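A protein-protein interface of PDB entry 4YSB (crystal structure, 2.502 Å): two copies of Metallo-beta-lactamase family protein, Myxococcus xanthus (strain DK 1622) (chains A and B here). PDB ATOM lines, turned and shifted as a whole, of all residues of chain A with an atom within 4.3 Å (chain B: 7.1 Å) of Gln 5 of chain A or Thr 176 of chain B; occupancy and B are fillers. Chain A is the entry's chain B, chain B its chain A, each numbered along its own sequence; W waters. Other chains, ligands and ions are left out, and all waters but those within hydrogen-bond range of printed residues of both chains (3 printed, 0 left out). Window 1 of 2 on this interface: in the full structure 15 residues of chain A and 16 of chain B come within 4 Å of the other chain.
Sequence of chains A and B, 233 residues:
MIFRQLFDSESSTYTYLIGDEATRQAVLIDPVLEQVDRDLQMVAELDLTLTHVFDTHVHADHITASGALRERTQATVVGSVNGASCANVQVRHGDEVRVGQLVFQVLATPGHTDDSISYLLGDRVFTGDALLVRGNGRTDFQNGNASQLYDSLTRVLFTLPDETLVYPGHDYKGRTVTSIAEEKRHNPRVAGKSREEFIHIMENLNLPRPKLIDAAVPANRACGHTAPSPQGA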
ATOM      1  N   ARG A   4      16.583 -11.500   1.178  1.00  0.00           N
ATOM      2  CA  ARG A   4      17.961 -11.892   1.450  1.00  0.00           C
ATOM      3  C   ARG A   4      18.601 -12.491   0.203  1.00  0.00           C
ATOM      4  O   ARG A   4      18.041 -13.392  -0.421  1.00  0.00           O
ATOM      5  CB  ARG A   4      18.025 -12.897   2.602  1.00  0.00           C
ATOM      6  CG  ARG A   4      17.702 -12.319   3.971  1.00  0.00           C
ATOM      7  CD  ARG A   4      18.768 -11.340   4.426  1.00  0.00           C
ATOM      8  NE  ARG A   4      18.535 -10.873   5.791  1.00  0.00           N
ATOM      9  CZ  ARG A   4      17.781  -9.826   6.104  1.00  0.00           C
ATOM     10  NH1 ARG A   4      17.182  -9.130   5.148  1.00  0.00           N
ATOM     11  NH2 ARG A   4      17.622  -9.475   7.373  1.00  0.00           N
ATOM     12  N   GLN A   5      19.774 -11.984  -0.160  1.00  0.00           N
ATOM     13  CA  GLN A   5      20.509 -12.503  -1.307  1.00  0.00           C
ATOM     14  C   GLN A   5      21.684 -13.352  -0.835  1.00  0.00           C
ATOM     15  O   GLN A   5      22.491 -12.904  -0.022  1.00  0.00           O
ATOM     16  CB  GLN A   5      20.994 -11.358  -2.198  1.00  0.00           C
ATOM     17  CG  GLN A   5      21.703 -11.807  -3.466  1.00  0.00           C
ATOM     18  CD  GLN A   5      22.043 -10.645  -4.380  1.00  0.00           C
ATOM     19  OE1 GLN A   5      21.999  -9.484  -3.971  1.00  0.00           O
ATOM     20  NE2 GLN A   5      22.378 -10.950  -5.629  1.00  0.00           N
ATOM     21  N   LEU A   6      21.771 -14.577  -1.339  1.00  0.00           N
ATOM     22  CA  LEU A   6      22.838 -15.489  -0.941  1.00  0.00           C
ATOM     23  C   LEU A   6      23.747 -15.825  -2.118  1.00  0.00           C
ATOM     24  O   LEU A   6      23.291 -15.929  -3.256  1.00  0.00           O
ATOM     25  CB  LEU A   6      22.250 -16.769  -0.346  1.00  0.00           C
ATOM     26  CG  LEU A   6      21.341 -16.586   0.870  1.00  0.00           C
ATOM     27  CD1 LEU A   6      20.715 -17.913   1.275  1.00  0.00           C
ATOM     28  CD2 LEU A   6      22.113 -15.979   2.028  1.00  0.00           C
ATOM     29  N   TYR A  14      23.584 -17.010  -7.416  1.00  0.00           N
ATOM     30  CA  TYR A  14      22.812 -16.214  -6.473  1.00  0.00           C
ATOM     31  C   TYR A  14      21.525 -16.930  -6.074  1.00  0.00           C
ATOM     32  O   TYR A  14      20.700 -17.264  -6.924  1.00  0.00           O
ATOM     33  CB  TYR A  14      22.485 -14.844  -7.067  1.00  0.00           C
ATOM     34  CG  TYR A  14      23.601 -13.834  -6.939  1.00  0.00           C
ATOM     35  CD1 TYR A  14      24.297 -13.687  -5.746  1.00  0.00           C
ATOM     36  CD2 TYR A  14      23.964 -13.032  -8.013  1.00  0.00           C
ATOM     37  CE1 TYR A  14      25.319 -12.764  -5.625  1.00  0.00           C
ATOM     38  CE2 TYR A  14      24.987 -12.108  -7.903  1.00  0.00           C
ATOM     39  CZ  TYR A  14      25.661 -11.979  -6.706  1.00  0.00           C
ATOM     40  OH  TYR A  14      26.679 -11.062  -6.589  1.00  0.00           O
ATOM     41  N   THR A  15      21.367 -17.172  -4.777  1.00  0.00           N
ATOM     42  CA  THR A  15      20.129 -17.721  -4.236  1.00  0.00           C
ATOM     43  C   THR A  15      19.334 -16.591  -3.593  1.00  0.00           C
ATOM     44  O   THR A  15      19.905 -15.733  -2.918  1.00  0.00           O
ATOM     45  CB  THR A  15      20.399 -18.833  -3.199  1.00  0.00           C
ATOM     46  OG1 THR A  15      21.115 -19.907  -3.820  1.00  0.00           O
ATOM     47  CG2 THR A  15      19.095 -19.370  -2.629  1.00  0.00           C
ATOM     48  N   TYR A  16      18.024 -16.580  -3.808  1.00  0.00           N
ATOM     49  CA  TYR A  16      17.193 -15.503  -3.283  1.00  0.00           C
ATOM     50  C   TYR A  16      16.127 -16.002  -2.315  1.00  0.00           C
ATOM     51  O   TYR A  16      15.330 -16.881  -2.640  1.00  0.00           O
ATOM     52  CB  TYR A  16      16.546 -14.732  -4.433  1.00  0.00           C
ATOM     53  CG  TYR A  16      17.560 -14.053  -5.322  1.00  0.00           C
ATOM     54  CD1 TYR A  16      18.134 -12.844  -4.948  1.00  0.00           C
ATOM     55  CD2 TYR A  16      17.960 -14.627  -6.522  1.00  0.00           C
ATOM     56  CE1 TYR A  16      19.071 -12.222  -5.748  1.00  0.00           C
ATOM     57  CE2 TYR A  16      18.895 -14.011  -7.329  1.00  0.00           C
ATOM     58  CZ  TYR A  16      19.449 -12.809  -6.938  1.00  0.00           C
ATOM     59  OH  TYR A  16      20.381 -12.191  -7.739  1.00  0.00           O
ATOM     60  N   TYR A 167      17.610  -9.078 -10.522  1.00  0.00           N
ATOM     61  CA  TYR A 167      18.449  -9.955  -9.717  1.00  0.00           C
ATOM     62  C   TYR A 167      18.825 -11.212 -10.499  1.00  0.00           C
ATOM     63  O   TYR A 167      18.006 -12.117 -10.662  1.00  0.00           O
ATOM     64  CB  TYR A 167      17.739 -10.323  -8.413  1.00  0.00           C
ATOM     65  CG  TYR A 167      17.674  -9.188  -7.413  1.00  0.00           C
ATOM     66  CD1 TYR A 167      18.758  -8.896  -6.596  1.00  0.00           C
ATOM     67  CD2 TYR A 167      16.531  -8.410  -7.286  1.00  0.00           C
ATOM     68  CE1 TYR A 167      18.707  -7.862  -5.680  1.00  0.00           C
ATOM     69  CE2 TYR A 167      16.470  -7.372  -6.373  1.00  0.00           C
ATOM     70  CZ  TYR A 167      17.561  -7.103  -5.573  1.00  0.00           C
ATOM     71  OH  TYR A 167      17.507  -6.071  -4.663  1.00  0.00           O
ATOM     72  N   THR A 176      25.841  -7.420  -7.652  1.00  0.00           N
ATOM     73  CA  THR A 176      24.734  -8.100  -6.987  1.00  0.00           C
ATOM     74  C   THR A 176      23.383  -7.815  -7.634  1.00  0.00           C
ATOM     75  O   THR A 176      22.464  -8.629  -7.545  1.00  0.00           O
ATOM     76  CB  THR A 176      24.654  -7.704  -5.499  1.00  0.00           C
ATOM     77  OG1 THR A 176      24.517  -6.283  -5.388  1.00  0.00           O
ATOM     78  CG2 THR A 176      25.908  -8.148  -4.762  1.00  0.00           C
ATOM     79  N   GLN B   5      25.624  -3.015  -3.496  1.00  0.00           N
ATOM     80  CA  GLN B   5      26.617  -3.779  -2.755  1.00  0.00           C
ATOM     81  C   GLN B   5      27.564  -4.467  -3.729  1.00  0.00           C
ATOM     82  O   GLN B   5      27.125  -5.175  -4.634  1.00  0.00           O
ATOM     83  CB  GLN B   5      25.944  -4.804  -1.840  1.00  0.00           C
ATOM     84  CG  GLN B   5      26.909  -5.580  -0.957  1.00  0.00           C
ATOM     85  CD  GLN B   5      26.198  -6.432   0.079  1.00  0.00           C
ATOM     86  OE1 GLN B   5      25.001  -6.691  -0.031  1.00  0.00           O
ATOM     87  NE2 GLN B   5      26.935  -6.865   1.096  1.00  0.00           N
ATOM     88  N   TYR B  14      33.332  -6.484   1.075  1.00  0.00           N
ATOM     89  CA  TYR B  14      32.131  -5.824   0.583  1.00  0.00           C
ATOM     90  C   TYR B  14      32.358  -4.324   0.417  1.00  0.00           C
ATOM     91  O   TYR B  14      32.737  -3.634   1.364  1.00  0.00           O
ATOM     92  CB  TYR B  14      30.955  -6.076   1.529  1.00  0.00           C
ATOM     93  CG  TYR B  14      30.247  -7.392   1.296  1.00  0.00           C
ATOM     94  CD1 TYR B  14      29.970  -7.836   0.011  1.00  0.00           C
ATOM     95  CD2 TYR B  14      29.862  -8.195   2.365  1.00  0.00           C
ATOM     96  CE1 TYR B  14      29.321  -9.039  -0.207  1.00  0.00           C
ATOM     97  CE2 TYR B  14      29.217  -9.400   2.156  1.00  0.00           C
ATOM     98  CZ  TYR B  14      28.949  -9.816   0.869  1.00  0.00           C
ATOM     99  OH  TYR B  14      28.307 -11.014   0.658  1.00  0.00           O
ATOM    100  N   TYR B  16      30.465  -0.729  -0.637  1.00  0.00           N
ATOM    101  CA  TYR B  16      29.111  -0.192  -0.673  1.00  0.00           C
ATOM    102  C   TYR B  16      29.037   1.157  -1.375  1.00  0.00           C
ATOM    103  O   TYR B  16      29.743   2.102  -1.021  1.00  0.00           O
ATOM    104  CB  TYR B  16      28.552  -0.080   0.743  1.00  0.00           C
ATOM    105  CG  TYR B  16      28.447  -1.415   1.439  1.00  0.00           C
ATOM    106  CD1 TYR B  16      27.366  -2.254   1.209  1.00  0.00           C
ATOM    107  CD2 TYR B  16      29.438  -1.844   2.314  1.00  0.00           C
ATOM    108  CE1 TYR B  16      27.269  -3.480   1.836  1.00  0.00           C
ATOM    109  CE2 TYR B  16      29.350  -3.067   2.946  1.00  0.00           C
ATOM    110  CZ  TYR B  16      28.264  -3.881   2.703  1.00  0.00           C
ATOM    111  OH  TYR B  16      28.174  -5.102   3.334  1.00  0.00           O
ATOM    112  N   VAL B 133      28.265 -10.978   9.785  1.00  0.00           N
ATOM    113  CA  VAL B 133      27.107 -11.859   9.762  1.00  0.00           C
ATOM    114  C   VAL B 133      27.401 -13.100  10.597  1.00  0.00           C
ATOM    115  O   VAL B 133      28.244 -13.917  10.223  1.00  0.00           O
ATOM    116  CB  VAL B 133      26.727 -12.277   8.331  1.00  0.00           C
ATOM    117  CG1 VAL B 133      25.510 -13.190   8.356  1.00  0.00           C
ATOM    118  CG2 VAL B 133      26.464 -11.051   7.471  1.00  0.00           C
ATOM    119  N   VAL B 166      22.398  -4.543   8.964  1.00  0.00           N
ATOM    120  CA  VAL B 166      23.840  -4.522   9.168  1.00  0.00           C
ATOM    121  C   VAL B 166      24.580  -4.978   7.917  1.00  0.00           C
ATOM    122  O   VAL B 166      24.435  -6.120   7.480  1.00  0.00           O
ATOM    123  CB  VAL B 166      24.253  -5.410  10.354  1.00  0.00           C
ATOM    124  CG1 VAL B 166      25.768  -5.475  10.466  1.00  0.00           C
ATOM    125  CG2 VAL B 166      23.635  -4.893  11.641  1.00  0.00           C
ATOM    126  N   TYR B 167      25.369  -4.075   7.344  1.00  0.00           N
ATOM    127  CA  TYR B 167      26.160  -4.385   6.161  1.00  0.00           C
ATOM    128  C   TYR B 167      27.644  -4.478   6.512  1.00  0.00           C
ATOM    129  O   TYR B 167      28.320  -3.459   6.655  1.00  0.00           O
ATOM    130  CB  TYR B 167      25.928  -3.335   5.073  1.00  0.00           C
ATOM    131  CG  TYR B 167      24.590  -3.460   4.376  1.00  0.00           C
ATOM    132  CD1 TYR B 167      24.384  -4.424   3.397  1.00  0.00           C
ATOM    133  CD2 TYR B 167      23.534  -2.616   4.695  1.00  0.00           C
ATOM    134  CE1 TYR B 167      23.165  -4.544   2.755  1.00  0.00           C
ATOM    135  CE2 TYR B 167      22.311  -2.731   4.059  1.00  0.00           C
ATOM    136  CZ  TYR B 167      22.132  -3.696   3.090  1.00  0.00           C
ATOM    137  OH  TYR B 167      20.917  -3.815   2.453  1.00  0.00           O
ATOM    138  N   PRO B 168      28.154  -5.712   6.648  1.00  0.00           N
ATOM    139  CA  PRO B 168      29.517  -5.982   7.115  1.00  0.00           C
ATOM    140  C   PRO B 168      30.579  -5.699   6.059  1.00  0.00           C
ATOM    141  O   PRO B 168      30.261  -5.573   4.877  1.00  0.00           O
ATOM    142  CB  PRO B 168      29.474  -7.473   7.447  1.00  0.00           C
ATOM    143  CG  PRO B 168      28.491  -8.020   6.478  1.00  0.00           C
ATOM    144  CD  PRO B 168      27.435  -6.954   6.312  1.00  0.00           C
ATOM    145  N   ASP B 171      32.468 -11.171   4.274  1.00  0.00           N
ATOM    146  CA  ASP B 171      31.777 -12.427   4.536  1.00  0.00           C
ATOM    147  C   ASP B 171      32.415 -13.515   3.687  1.00  0.00           C
ATOM    148  O   ASP B 171      32.767 -13.285   2.530  1.00  0.00           O
ATOM    149  CB  ASP B 171      30.279 -12.325   4.243  1.00  0.00           C
ATOM    150  CG  ASP B 171      29.494 -13.482   4.836  1.00  0.00           C
ATOM    151  OD1 ASP B 171      29.082 -13.383   6.011  1.00  0.00           O
ATOM    152  OD2 ASP B 171      29.295 -14.495   4.133  1.00  0.00           O
ATOM    153  N   LYS B 173      31.030 -16.769   3.566  1.00  0.00           N
ATOM    154  CA  LYS B 173      30.059 -17.849   3.419  1.00  0.00           C
ATOM    155  C   LYS B 173      28.867 -17.460   2.545  1.00  0.00           C
ATOM    156  O   LYS B 173      27.887 -18.199   2.458  1.00  0.00           O
ATOM    157  CB  LYS B 173      29.573 -18.310   4.795  1.00  0.00           C
ATOM    158  CG  LYS B 173      30.639 -19.028   5.609  1.00  0.00           C
ATOM    159  CD  LYS B 173      30.271 -20.484   5.841  1.00  0.00           C
ATOM    160  CE  LYS B 173      29.250 -20.625   6.958  1.00  0.00           C
ATOM    161  NZ  LYS B 173      29.821 -20.241   8.279  1.00  0.00           N
ATOM    162  N   GLY B 174      28.951 -16.297   1.905  1.00  0.00           N
ATOM    163  CA  GLY B 174      27.951 -15.894   0.932  1.00  0.00           C
ATOM    164  C   GLY B 174      26.783 -15.090   1.471  1.00  0.00           C
ATOM    165  O   GLY B 174      25.823 -14.826   0.746  1.00  0.00           O
ATOM    166  N   ARG B 175      26.852 -14.703   2.740  1.00  0.00           N
ATOM    167  CA  ARG B 175      25.826 -13.846   3.323  1.00  0.00           C
ATOM    168  C   ARG B 175      26.128 -12.392   2.988  1.00  0.00           C
ATOM    169  O   ARG B 175      27.281 -11.965   3.037  1.00  0.00           O
ATOM    170  CB  ARG B 175      25.737 -14.038   4.839  1.00  0.00           C
ATOM    171  CG  ARG B 175      25.103 -15.353   5.282  1.00  0.00           C
ATOM    172  CD  ARG B 175      26.109 -16.492   5.280  1.00  0.00           C
ATOM    173  NE  ARG B 175      27.349 -16.112   5.950  1.00  0.00           N
ATOM    174  CZ  ARG B 175      27.586 -16.291   7.246  1.00  0.00           C
ATOM    175  NH1 ARG B 175      28.744 -15.911   7.767  1.00  0.00           N
ATOM    176  NH2 ARG B 175      26.668 -16.853   8.022  1.00  0.00           N
ATOM    177  N   THR B 176      25.091 -11.633   2.648  1.00  0.00           N
ATOM    178  CA  THR B 176      25.276 -10.259   2.194  1.00  0.00           C
ATOM    179  C   THR B 176      24.847  -9.229   3.236  1.00  0.00           C
ATOM    180  O   THR B 176      25.343  -8.102   3.242  1.00  0.00           O
ATOM    181  CB  THR B 176      24.497  -9.995   0.892  1.00  0.00           C
ATOM    182  OG1 THR B 176      23.101 -10.229   1.111  1.00  0.00           O
ATOM    183  CG2 THR B 176      24.993 -10.909  -0.219  1.00  0.00           C
ATOM    184  N   VAL B 177      23.930  -9.616   4.116  1.00  0.00           N
ATOM    185  CA  VAL B 177      23.382  -8.683   5.093  1.00  0.00           C
ATOM    186  C   VAL B 177      22.777  -9.414   6.290  1.00  0.00           C
ATOM    187  O   VAL B 177      22.312 -10.547   6.172  1.00  0.00           O
ATOM    188  CB  VAL B 177      22.308  -7.764   4.447  1.00  0.00           C
ATOM    189  CG1 VAL B 177      21.062  -8.557   4.089  1.00  0.00           C
ATOM    190  CG2 VAL B 177      21.957  -6.595   5.360  1.00  0.00           C
ATOM    191  N   THR B 178      22.813  -8.763   7.447  1.00  0.00           N
ATOM    192  CA  THR B 178      22.106  -9.236   8.629  1.00  0.00           C
ATOM    193  C   THR B 178      21.410  -8.052   9.291  1.00  0.00           C
ATOM    194  O   THR B 178      21.346  -6.965   8.716  1.00  0.00           O
ATOM    195  CB  THR B 178      23.052  -9.921   9.631  1.00  0.00           C
ATOM    196  OG1 THR B 178      22.335 -10.236  10.830  1.00  0.00           O
ATOM    197  CG2 THR B 178      24.221  -9.012   9.971  1.00  0.00           C
HETATM  198  O   HOH W   1      20.370  -8.978   0.350  1.00  0.00           O
HETATM  199  O   HOH W   2      22.883  -4.603  -3.480  1.00  0.00           O
HETATM  200  O   HOH W   3      20.323 -12.440   7.716  1.00  0.00           O
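OG1 of Thr 176 of chain B sits at hydrogen-bond distance from O of Gln 5 of chain A (3.0 Å).
The backbone carbonyl oxygen of Gln 5 of chain B is in hydrogen-bond range of the side-chain hydroxyl of Thr 176 of chain A (2.9 Å).
The backbone carbonyl oxygen (O) of Thr 15 of chain A sits at hydrogen-bond distance from the backbone NH (N) of Leu 6 of chain A (2.7 Å).
The side-chain carboxylate of Asp 171 of chain B lies within hydrogen-bond range of the backbone NH of Gly 174 of chain B, at 2.9 Å.
NE2 of Gln 5 of chain B is in hydrogen-bond range of OH of Tyr 16 of chain B.
The side-chain amide nitrogen of Gln 5 of chain A is in hydrogen-bond range of the side-chain hydroxyl of Tyr 16 of chain A (3.2 Å).
O of Thr 176 of chain A sits at hydrogen-bond distance from NE2 of Gln 5 of chain A (3.0 Å).
The side-chain amide nitrogen (NE2) of Gln 5 of chain B sits at hydrogen-bond distance from the backbone carbonyl oxygen (O) of Thr 176 of chain B.
Among the printed residues, pairs that only touch across the chains: Arg 4 of chain A with Val 177 of chain B (3.6 Å), Gln 5 of chain A with Gly 174 of chain B (3.9 Å) and Leu 6 of chain A with Gly 174 of chain B (3.5 Å).
Of the printed residues of chain B, Arg 4 of chain A touches Val 177 (3.6 Å).
Gln 5 of chain A touches just these residues of chain B: Gly 174 (3.9 Å) and Thr 176 (3.0 Å).
Of the printed residues of chain B, Leu 6 of chain A touches Gly 174.
Printed residues of chain B within 4 Å of Thr 176 of chain A: Gln 5 (2.9 Å).
Printed residues of chain A within 4 Å of Gly 174 of chain B: Gln 5 (3.9 Å) and Leu 6 (3.5 Å).
Thr 176 of chain B touches just one residue of chain A: Gln 5.
Printed residues of chain A within 4 Å of Val 177 of chain B: Arg 4 (3.6 Å).
The nearest printed residue of chain A that does not touch Thr 176 of chain B is Leu 6 of chain A (5.0 Å).
The nearest printed residue of chain B that does not touch Thr 176 of chain A is Thr 176 of chain B (5.4 Å).
Hydrophobic or aromatic side chains of chain B within 4 Å of the printed part of chain A: Val 177.
Gln 5 of chain A touches Thr 176 of chain B, and with the chains exchanged Thr 176 of chain A touches Gln 5 of chain B.
Positions printed for both chains: 5, 14, 16, 167 and 176.
Of the 5 pairs that touch across the chains among the printed residues, 2 have their exchanged pair printed and touching as well.
Water W2 lies within hydrogen-bond range of OG1 of Thr 176 of chain A (3.0 Å) and N of Gln 5 of chain B (3.2 Å).
Water W3 lies within hydrogen-bond range of NE of Arg 4 of chain A and O of Val 177 of chain B.
Water W1 lies within hydrogen-bond range of OG1 of Thr 176 of chain B (3.1 Å) and N of Gln 5 of chain A (3.1 Å).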
